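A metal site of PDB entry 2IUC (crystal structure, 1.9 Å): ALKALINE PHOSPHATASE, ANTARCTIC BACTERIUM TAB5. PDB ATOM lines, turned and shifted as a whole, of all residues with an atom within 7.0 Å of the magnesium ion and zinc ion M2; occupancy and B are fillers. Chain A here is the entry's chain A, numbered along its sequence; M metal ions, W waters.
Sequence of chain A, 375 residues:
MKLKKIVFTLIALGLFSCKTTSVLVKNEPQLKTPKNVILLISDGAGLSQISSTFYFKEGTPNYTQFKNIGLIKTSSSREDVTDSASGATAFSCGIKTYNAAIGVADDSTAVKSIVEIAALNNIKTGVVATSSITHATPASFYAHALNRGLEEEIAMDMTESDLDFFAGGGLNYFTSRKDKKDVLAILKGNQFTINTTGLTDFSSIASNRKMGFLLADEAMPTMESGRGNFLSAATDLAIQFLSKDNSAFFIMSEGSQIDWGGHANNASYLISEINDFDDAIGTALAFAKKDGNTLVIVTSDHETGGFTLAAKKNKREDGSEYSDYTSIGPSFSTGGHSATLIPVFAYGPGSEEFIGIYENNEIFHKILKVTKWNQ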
ATOM      1  N   ILE A  41       0.125   7.482 -14.433  1.00  0.00           N
ATOM      2  CA  ILE A  41      -1.066   8.083 -15.041  1.00  0.00           C
ATOM      3  C   ILE A  41      -1.099   7.537 -16.424  1.00  0.00           C
ATOM      4  O   ILE A  41      -0.105   7.678 -17.197  1.00  0.00           O
ATOM      5  CB  ILE A  41      -0.942   9.673 -15.081  1.00  0.00           C
ATOM      6  CG1 ILE A  41      -0.831  10.249 -13.671  1.00  0.00           C
ATOM      7  CG2 ILE A  41      -2.090  10.287 -15.991  1.00  0.00           C
ATOM      8  CD1 ILE A  41      -0.568  11.782 -13.639  1.00  0.00           C
ATOM      9  N   SER A  42      -2.205   6.861 -16.768  1.00  0.00           N
ATOM     10  CA  SER A  42      -2.410   6.361 -18.112  1.00  0.00           C
ATOM     11  C   SER A  42      -3.337   7.435 -18.737  1.00  0.00           C
ATOM     12  O   SER A  42      -4.547   7.517 -18.426  1.00  0.00           O
ATOM     13  CB  SER A  42      -3.100   5.026 -18.036  1.00  0.00           C
ATOM     14  OG  SER A  42      -4.110   5.106 -17.016  1.00  0.00           O
ATOM     15  N   ASP A  43      -2.767   8.238 -19.612  1.00  0.00           N
ATOM     16  CA  ASP A  43      -3.550   9.270 -20.243  1.00  0.00           C
ATOM     17  C   ASP A  43      -4.623   8.739 -21.127  1.00  0.00           C
ATOM     18  O   ASP A  43      -4.333   8.012 -22.085  1.00  0.00           O
ATOM     19  CB  ASP A  43      -2.655  10.190 -21.069  1.00  0.00           C
ATOM     20  CG  ASP A  43      -3.330  11.574 -21.338  1.00  0.00           C
ATOM     21  OD1 ASP A  43      -4.427  11.626 -21.842  1.00  0.00           O
ATOM     22  OD2 ASP A  43      -2.743  12.617 -21.015  1.00  0.00           O
ATOM     23  N   GLY A  44      -5.879   9.102 -20.831  1.00  0.00           N
ATOM     24  CA  GLY A  44      -6.969   8.687 -21.706  1.00  0.00           C
ATOM     25  C   GLY A  44      -7.513   7.281 -21.544  1.00  0.00           C
ATOM     26  O   GLY A  44      -8.257   6.841 -22.395  1.00  0.00           O
ATOM     27  N   THR A  82     -13.042  17.135 -19.345  1.00  0.00           N
ATOM     28  CA  THR A  82     -11.778  17.740 -19.029  1.00  0.00           C
ATOM     29  C   THR A  82     -10.795  17.518 -20.190  1.00  0.00           C
ATOM     30  O   THR A  82     -10.999  16.620 -21.004  1.00  0.00           O
ATOM     31  CB  THR A  82     -11.172  17.070 -17.750  1.00  0.00           C
ATOM     32  OG1 THR A  82     -10.044  17.851 -17.318  1.00  0.00           O
ATOM     33  CG2 THR A  82     -10.673  15.683 -18.098  1.00  0.00           C
ATOM     34  N   ASP A  83      -9.752  18.310 -20.248  1.00  0.00           N
ATOM     35  CA  ASP A  83      -8.565  17.935 -21.068  1.00  0.00           C
ATOM     36  C   ASP A  83      -7.453  17.458 -20.132  1.00  0.00           C
ATOM     37  O   ASP A  83      -7.609  17.443 -18.895  1.00  0.00           O
ATOM     38  CB  ASP A  83      -8.124  19.126 -22.004  1.00  0.00           C
ATOM     39  CG  ASP A  83      -7.262  20.183 -21.300  1.00  0.00           C
ATOM     40  OD1 ASP A  83      -7.349  20.447 -20.057  1.00  0.00           O
ATOM     41  OD2 ASP A  83      -6.478  20.823 -22.021  1.00  0.00           O
ATOM     42  N   SER A  84      -6.303  17.127 -20.701  1.00  0.00           N
ATOM     43  CA  SER A  84      -5.213  16.595 -19.860  1.00  0.00           C
ATOM     44  C   SER A  84      -4.611  17.627 -18.921  1.00  0.00           C
ATOM     45  O   SER A  84      -3.992  17.298 -17.867  1.00  0.00           O
ATOM     46  CB  SER A  84      -4.085  16.229 -20.797  1.00  0.00           C
ATOM     47  OG  SER A  84      -4.545  15.164 -21.562  1.00  0.00           O
ATOM     48  N   ALA A  85      -4.677  18.901 -19.352  1.00  0.00           N
ATOM     49  CA  ALA A  85      -4.044  19.985 -18.588  1.00  0.00           C
ATOM     50  C   ALA A  85      -4.764  20.177 -17.243  1.00  0.00           C
ATOM     51  O   ALA A  85      -4.074  20.160 -16.165  1.00  0.00           O
ATOM     52  CB  ALA A  85      -4.047  21.253 -19.366  1.00  0.00           C
ATOM     53  N   GLY A  87      -6.930  18.154 -15.936  1.00  0.00           N
ATOM     54  CA  GLY A  87      -6.915  16.784 -15.397  1.00  0.00           C
ATOM     55  C   GLY A  87      -5.674  16.525 -14.566  1.00  0.00           C
ATOM     56  O   GLY A  87      -5.787  16.030 -13.497  1.00  0.00           O
ATOM     57  N   ALA A  88      -4.494  16.833 -15.091  1.00  0.00           N
ATOM     58  CA  ALA A  88      -3.299  16.566 -14.370  1.00  0.00           C
ATOM     59  C   ALA A  88      -3.069  17.616 -13.263  1.00  0.00           C
ATOM     60  O   ALA A  88      -2.385  17.304 -12.285  1.00  0.00           O
ATOM     61  CB  ALA A  88      -2.133  16.600 -15.279  1.00  0.00           C
ATOM     62  N   SER A 131       5.381  11.009 -24.087  1.00  0.00           N
ATOM     63  CA  SER A 131       5.211  12.193 -24.939  1.00  0.00           C
ATOM     64  C   SER A 131       6.445  13.065 -24.786  1.00  0.00           C
ATOM     65  O   SER A 131       7.444  12.684 -24.095  1.00  0.00           O
ATOM     66  CB  SER A 131       3.963  12.966 -24.466  1.00  0.00           C
ATOM     67  OG  SER A 131       4.187  13.373 -23.123  1.00  0.00           O
ATOM     68  N   HIS A 135       4.703  18.115 -22.583  1.00  0.00           N
ATOM     69  CA  HIS A 135       3.257  17.821 -22.831  1.00  0.00           C
ATOM     70  C   HIS A 135       2.431  18.046 -21.525  1.00  0.00           C
ATOM     71  O   HIS A 135       3.017  18.135 -20.483  1.00  0.00           O
ATOM     72  CB  HIS A 135       3.029  16.385 -23.380  1.00  0.00           C
ATOM     73  CG  HIS A 135       1.861  16.300 -24.326  1.00  0.00           C
ATOM     74  ND1 HIS A 135       0.632  15.795 -23.943  1.00  0.00           N
ATOM     75  CD2 HIS A 135       1.725  16.695 -25.631  1.00  0.00           C
ATOM     76  CE1 HIS A 135      -0.207  15.892 -24.973  1.00  0.00           C
ATOM     77  NE2 HIS A 135       0.437  16.423 -26.008  1.00  0.00           N
ATOM     78  N   ALA A 136       1.118  18.180 -21.619  1.00  0.00           N
ATOM     79  CA  ALA A 136       0.345  18.768 -20.534  1.00  0.00           C
ATOM     80  C   ALA A 136       0.479  17.981 -19.203  1.00  0.00           C
ATOM     81  O   ALA A 136       0.458  18.530 -18.102  1.00  0.00           O
ATOM     82  CB  ALA A 136      -1.044  18.812 -20.970  1.00  0.00           C
ATOM     83  N   THR A 137       0.572  16.670 -19.305  1.00  0.00           N
ATOM     84  CA  THR A 137       0.560  15.830 -18.054  1.00  0.00           C
ATOM     85  C   THR A 137       1.834  16.028 -17.255  1.00  0.00           C
ATOM     86  O   THR A 137       1.759  16.479 -16.110  1.00  0.00           O
ATOM     87  CB  THR A 137       0.204  14.352 -18.370  1.00  0.00           C
ATOM     88  OG1 THR A 137      -1.028  14.293 -19.118  1.00  0.00           O
ATOM     89  CG2 THR A 137       0.131  13.469 -17.106  1.00  0.00           C
ATOM     90  N   PRO A 138       3.046  15.711 -17.869  1.00  0.00           N
ATOM     91  CA  PRO A 138       4.270  15.999 -17.087  1.00  0.00           C
ATOM     92  C   PRO A 138       4.420  17.465 -16.685  1.00  0.00           C
ATOM     93  O   PRO A 138       4.935  17.809 -15.581  1.00  0.00           O
ATOM     94  CB  PRO A 138       5.418  15.551 -18.045  1.00  0.00           C
ATOM     95  CG  PRO A 138       4.823  15.379 -19.421  1.00  0.00           C
ATOM     96  CD  PRO A 138       3.335  15.176 -19.223  1.00  0.00           C
ATOM     97  N   ARG A 148      -1.522  25.295 -21.960  1.00  0.00           N
ATOM     98  CA  ARG A 148      -0.678  24.127 -22.187  1.00  0.00           C
ATOM     99  C   ARG A 148       0.063  24.215 -23.502  1.00  0.00           C
ATOM    100  O   ARG A 148       0.993  23.468 -23.687  1.00  0.00           O
ATOM    101  CB  ARG A 148      -1.574  22.873 -22.313  1.00  0.00           C
ATOM    102  CG  ARG A 148      -2.629  22.977 -23.464  1.00  0.00           C
ATOM    103  CD  ARG A 148      -3.482  21.789 -23.352  1.00  0.00           C
ATOM    104  NE  ARG A 148      -2.751  20.564 -23.728  1.00  0.00           N
ATOM    105  CZ  ARG A 148      -3.294  19.342 -23.785  1.00  0.00           C
ATOM    106  NH1 ARG A 148      -4.596  19.173 -23.393  1.00  0.00           N
ATOM    107  NH2 ARG A 148      -2.552  18.294 -24.192  1.00  0.00           N
ATOM    108  N   GLU A 254       4.122   8.584 -16.778  1.00  0.00           N
ATOM    109  CA  GLU A 254       2.909   8.688 -17.573  1.00  0.00           C
ATOM    110  C   GLU A 254       3.001   7.792 -18.807  1.00  0.00           C
ATOM    111  O   GLU A 254       4.000   7.887 -19.585  1.00  0.00           O
ATOM    112  CB  GLU A 254       2.699  10.140 -18.070  1.00  0.00           C
ATOM    113  CG  GLU A 254       1.299  10.191 -18.741  1.00  0.00           C
ATOM    114  CD  GLU A 254       1.159  11.354 -19.723  1.00  0.00           C
ATOM    115  OE1 GLU A 254       2.173  11.950 -20.120  1.00  0.00           O
ATOM    116  OE2 GLU A 254       0.020  11.672 -20.058  1.00  0.00           O
ATOM    117  N   GLY A 255       1.992   6.932 -18.979  1.00  0.00           N
ATOM    118  CA  GLY A 255       1.682   6.228 -20.276  1.00  0.00           C
ATOM    119  C   GLY A 255       0.917   7.216 -21.197  1.00  0.00           C
ATOM    120  O   GLY A 255      -0.328   7.228 -21.224  1.00  0.00           O
ATOM    121  N   SER A 256       1.670   8.110 -21.843  1.00  0.00           N
ATOM    122  CA  SER A 256       1.139   9.294 -22.585  1.00  0.00           C
ATOM    123  C   SER A 256       0.361   9.001 -23.833  1.00  0.00           C
ATOM    124  O   SER A 256      -0.573   9.782 -24.199  1.00  0.00           O
ATOM    125  CB  SER A 256       2.288  10.248 -22.983  1.00  0.00           C
ATOM    126  OG  SER A 256       3.189  10.392 -21.924  1.00  0.00           O
ATOM    127  N   GLN A 257       0.722   7.919 -24.528  1.00  0.00           N
ATOM    128  CA  GLN A 257       0.242   7.755 -25.919  1.00  0.00           C
ATOM    129  C   GLN A 257      -1.016   6.910 -25.986  1.00  0.00           C
ATOM    130  O   GLN A 257      -1.656   6.764 -27.048  1.00  0.00           O
ATOM    131  CB  GLN A 257       1.362   7.185 -26.810  1.00  0.00           C
ATOM    132  CG  GLN A 257       2.535   8.176 -26.823  1.00  0.00           C
ATOM    133  CD  GLN A 257       3.530   7.813 -27.926  1.00  0.00           C
ATOM    134  OE1 GLN A 257       3.134   7.307 -28.952  1.00  0.00           O
ATOM    135  NE2 GLN A 257       4.819   8.136 -27.727  1.00  0.00           N
ATOM    136  N   ASP A 259      -3.837   7.844 -24.926  1.00  0.00           N
ATOM    137  CA  ASP A 259      -4.846   8.843 -25.359  1.00  0.00           C
ATOM    138  C   ASP A 259      -4.724   9.099 -26.878  1.00  0.00           C
ATOM    139  O   ASP A 259      -5.691   9.379 -27.600  1.00  0.00           O
ATOM    140  CB  ASP A 259      -4.502  10.105 -24.589  1.00  0.00           C
ATOM    141  CG  ASP A 259      -5.276  11.331 -25.107  1.00  0.00           C
ATOM    142  OD1 ASP A 259      -6.453  11.458 -24.748  1.00  0.00           O
ATOM    143  OD2 ASP A 259      -4.674  12.159 -25.831  1.00  0.00           O
ATOM    144  N   TRP A 260      -3.510   9.010 -27.400  1.00  0.00           N
ATOM    145  CA  TRP A 260      -3.359   9.368 -28.837  1.00  0.00           C
ATOM    146  C   TRP A 260      -3.946   8.302 -29.697  1.00  0.00           C
ATOM    147  O   TRP A 260      -4.474   8.593 -30.757  1.00  0.00           O
ATOM    148  CB  TRP A 260      -1.888   9.665 -29.203  1.00  0.00           C
ATOM    149  CG  TRP A 260      -1.226  10.769 -28.322  1.00  0.00           C
ATOM    150  CD1 TRP A 260      -1.855  11.600 -27.382  1.00  0.00           C
ATOM    151  CD2 TRP A 260       0.151  11.154 -28.331  1.00  0.00           C
ATOM    152  NE1 TRP A 260      -0.938  12.458 -26.829  1.00  0.00           N
ATOM    153  CE2 TRP A 260       0.310  12.220 -27.405  1.00  0.00           C
ATOM    154  CE3 TRP A 260       1.275  10.732 -29.077  1.00  0.00           C
ATOM    155  CZ2 TRP A 260       1.545  12.826 -27.168  1.00  0.00           C
ATOM    156  CZ3 TRP A 260       2.508  11.315 -28.849  1.00  0.00           C
ATOM    157  CH2 TRP A 260       2.637  12.371 -27.935  1.00  0.00           C
ATOM    158  N   HIS A 263      -7.748   9.039 -29.638  1.00  0.00           N
ATOM    159  CA  HIS A 263      -8.086  10.148 -30.552  1.00  0.00           C
ATOM    160  C   HIS A 263      -8.021   9.675 -31.981  1.00  0.00           C
ATOM    161  O   HIS A 263      -8.797  10.147 -32.788  1.00  0.00           O
ATOM    162  CB  HIS A 263      -7.093  11.320 -30.439  1.00  0.00           C
ATOM    163  CG  HIS A 263      -7.329  12.218 -29.258  1.00  0.00           C
ATOM    164  ND1 HIS A 263      -8.534  12.881 -29.034  1.00  0.00           N
ATOM    165  CD2 HIS A 263      -6.490  12.615 -28.267  1.00  0.00           C
ATOM    166  CE1 HIS A 263      -8.432  13.620 -27.938  1.00  0.00           C
ATOM    167  NE2 HIS A 263      -7.197  13.487 -27.464  1.00  0.00           N
ATOM    168  N   ASP A 301      -6.249  10.522 -16.352  1.00  0.00           N
ATOM    169  CA  ASP A 301      -6.896  11.833 -16.310  1.00  0.00           C
ATOM    170  C   ASP A 301      -8.359  11.901 -16.794  1.00  0.00           C
ATOM    171  O   ASP A 301      -9.121  12.765 -16.329  1.00  0.00           O
ATOM    172  CB  ASP A 301      -6.038  12.901 -17.005  1.00  0.00           C
ATOM    173  CG  ASP A 301      -5.616  12.516 -18.462  1.00  0.00           C
ATOM    174  OD1 ASP A 301      -5.900  11.412 -18.997  1.00  0.00           O
ATOM    175  OD2 ASP A 301      -5.097  13.420 -19.156  1.00  0.00           O
ATOM    176  N   HIS A 302      -8.752  11.040 -17.742  1.00  0.00           N
ATOM    177  CA  HIS A 302     -10.097  11.015 -18.350  1.00  0.00           C
ATOM    178  C   HIS A 302      -9.980   9.848 -19.362  1.00  0.00           C
ATOM    179  O   HIS A 302      -8.883   9.268 -19.555  1.00  0.00           O
ATOM    180  CB  HIS A 302     -10.390  12.367 -19.116  1.00  0.00           C
ATOM    181  CG  HIS A 302      -9.316  12.653 -20.142  1.00  0.00           C
ATOM    182  ND1 HIS A 302      -9.226  11.951 -21.319  1.00  0.00           N
ATOM    183  CD2 HIS A 302      -8.213  13.428 -20.093  1.00  0.00           C
ATOM    184  CE1 HIS A 302      -8.119  12.253 -21.940  1.00  0.00           C
ATOM    185  NE2 HIS A 302      -7.500  13.166 -21.245  1.00  0.00           N
ATOM    186  N   THR A 304     -10.670   8.442 -23.381  1.00  0.00           N
ATOM    187  CA  THR A 304     -10.737   8.961 -24.771  1.00  0.00           C
ATOM    188  C   THR A 304     -11.251   7.981 -25.852  1.00  0.00           C
ATOM    189  O   THR A 304     -10.814   6.797 -25.949  1.00  0.00           O
ATOM    190  CB  THR A 304      -9.337   9.357 -25.259  1.00  0.00           C
ATOM    191  OG1 THR A 304      -8.747  10.221 -24.325  1.00  0.00           O
ATOM    192  CG2 THR A 304      -9.423  10.122 -26.699  1.00  0.00           C
ATOM    193  N   HIS A 337     -12.381  13.318 -25.803  1.00  0.00           N
ATOM    194  CA  HIS A 337     -12.386  12.816 -24.406  1.00  0.00           C
ATOM    195  C   HIS A 337     -13.824  12.522 -24.021  1.00  0.00           C
ATOM    196  O   HIS A 337     -14.774  12.936 -24.716  1.00  0.00           O
ATOM    197  CB  HIS A 337     -11.776  13.895 -23.480  1.00  0.00           C
ATOM    198  CG  HIS A 337     -10.322  14.175 -23.748  1.00  0.00           C
ATOM    199  ND1 HIS A 337      -9.638  15.188 -23.116  1.00  0.00           N
ATOM    200  CD2 HIS A 337      -9.436  13.615 -24.640  1.00  0.00           C
ATOM    201  CE1 HIS A 337      -8.381  15.238 -23.586  1.00  0.00           C
ATOM    202  NE2 HIS A 337      -8.231  14.250 -24.450  1.00  0.00           N
HETATM  203 MG    MG M   1      -0.808  13.302 -21.229  1.00  0.00          MG
HETATM  204 ZN    ZN M   2      -5.377  13.352 -21.238  1.00  0.00          ZN
HETATM  205 ZN    ZN M   3      -6.538  13.668 -25.458  1.00  0.00          ZN
HETATM  206  O   HOH W   1      -1.472  15.208 -22.101  1.00  0.00           O
HETATM  207  O   HOH W   2       1.228  14.050 -21.717  1.00  0.00           O
HETATM  208  O   HOH W   3      -0.889  12.313 -23.086  1.00  0.00           O
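The magnesium ion is bound by the side-chain carboxylate (OD2) of Asp 43, water W3, the side-chain carboxylate (OE2) of Glu 254, water W1, water W2 and the side-chain hydroxyl (OG1) of Thr 137.
The magnesium ion has six donor atoms within binding distance.
ND1 of His 135 touches the magnesium ion, 3.96 Å away.
Within 4 Å of the magnesium ion: Asp 43, His 135, Thr 137 and Glu 254.
The nearest printed residue that does not touch the magnesium ion is Ser 84 (4.2 Å).
The nearest printed residue that does not touch zinc ion M2 is Asp 259 (4.1 Å).
Zinc ion M2 is bound by the side-chain hydroxyl (OG) of Ser 84 (2.0 Å), the side-chain carboxylate (OD1) of Asp 43 (2.1 Å), the side-chain carboxylate (OD2) of Asp 301 (2.1 Å) and a ring nitrogen (NE2) of His 302 (2.1 Å).
Slightly farther from zinc ion M2 lies the side-chain carboxylate (OD2) of Asp 43 (2.7 Å).
Water W2 lies within hydrogen-bond range of OE1 of Glu 254 (2.8 Å), ND1 of His 135 (2.9 Å) and OG of Ser 131 (3.3 Å).
O of Asp 43 is in hydrogen-bond range of N of Asp 259 (2.9 Å).
The backbone NH (N) of Asp 43 is in hydrogen-bond range of the backbone carbonyl oxygen (O) of Gly 255, at 3.1 Å.
OD1 of Asp 301 lies within hydrogen-bond range of N of Gly 44 (2.9 Å).
ND1 of His 337 lies close to NE2 of His 302 (3.5 Å).
The backbone NH of Gly 44 lies close to the backbone carbonyl oxygen of His 302 (3.3 Å).
The side-chain carboxylate (OE1) of Glu 254 lies within hydrogen-bond range of the side-chain hydroxyl (OG) of Ser 256 (2.6 Å).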
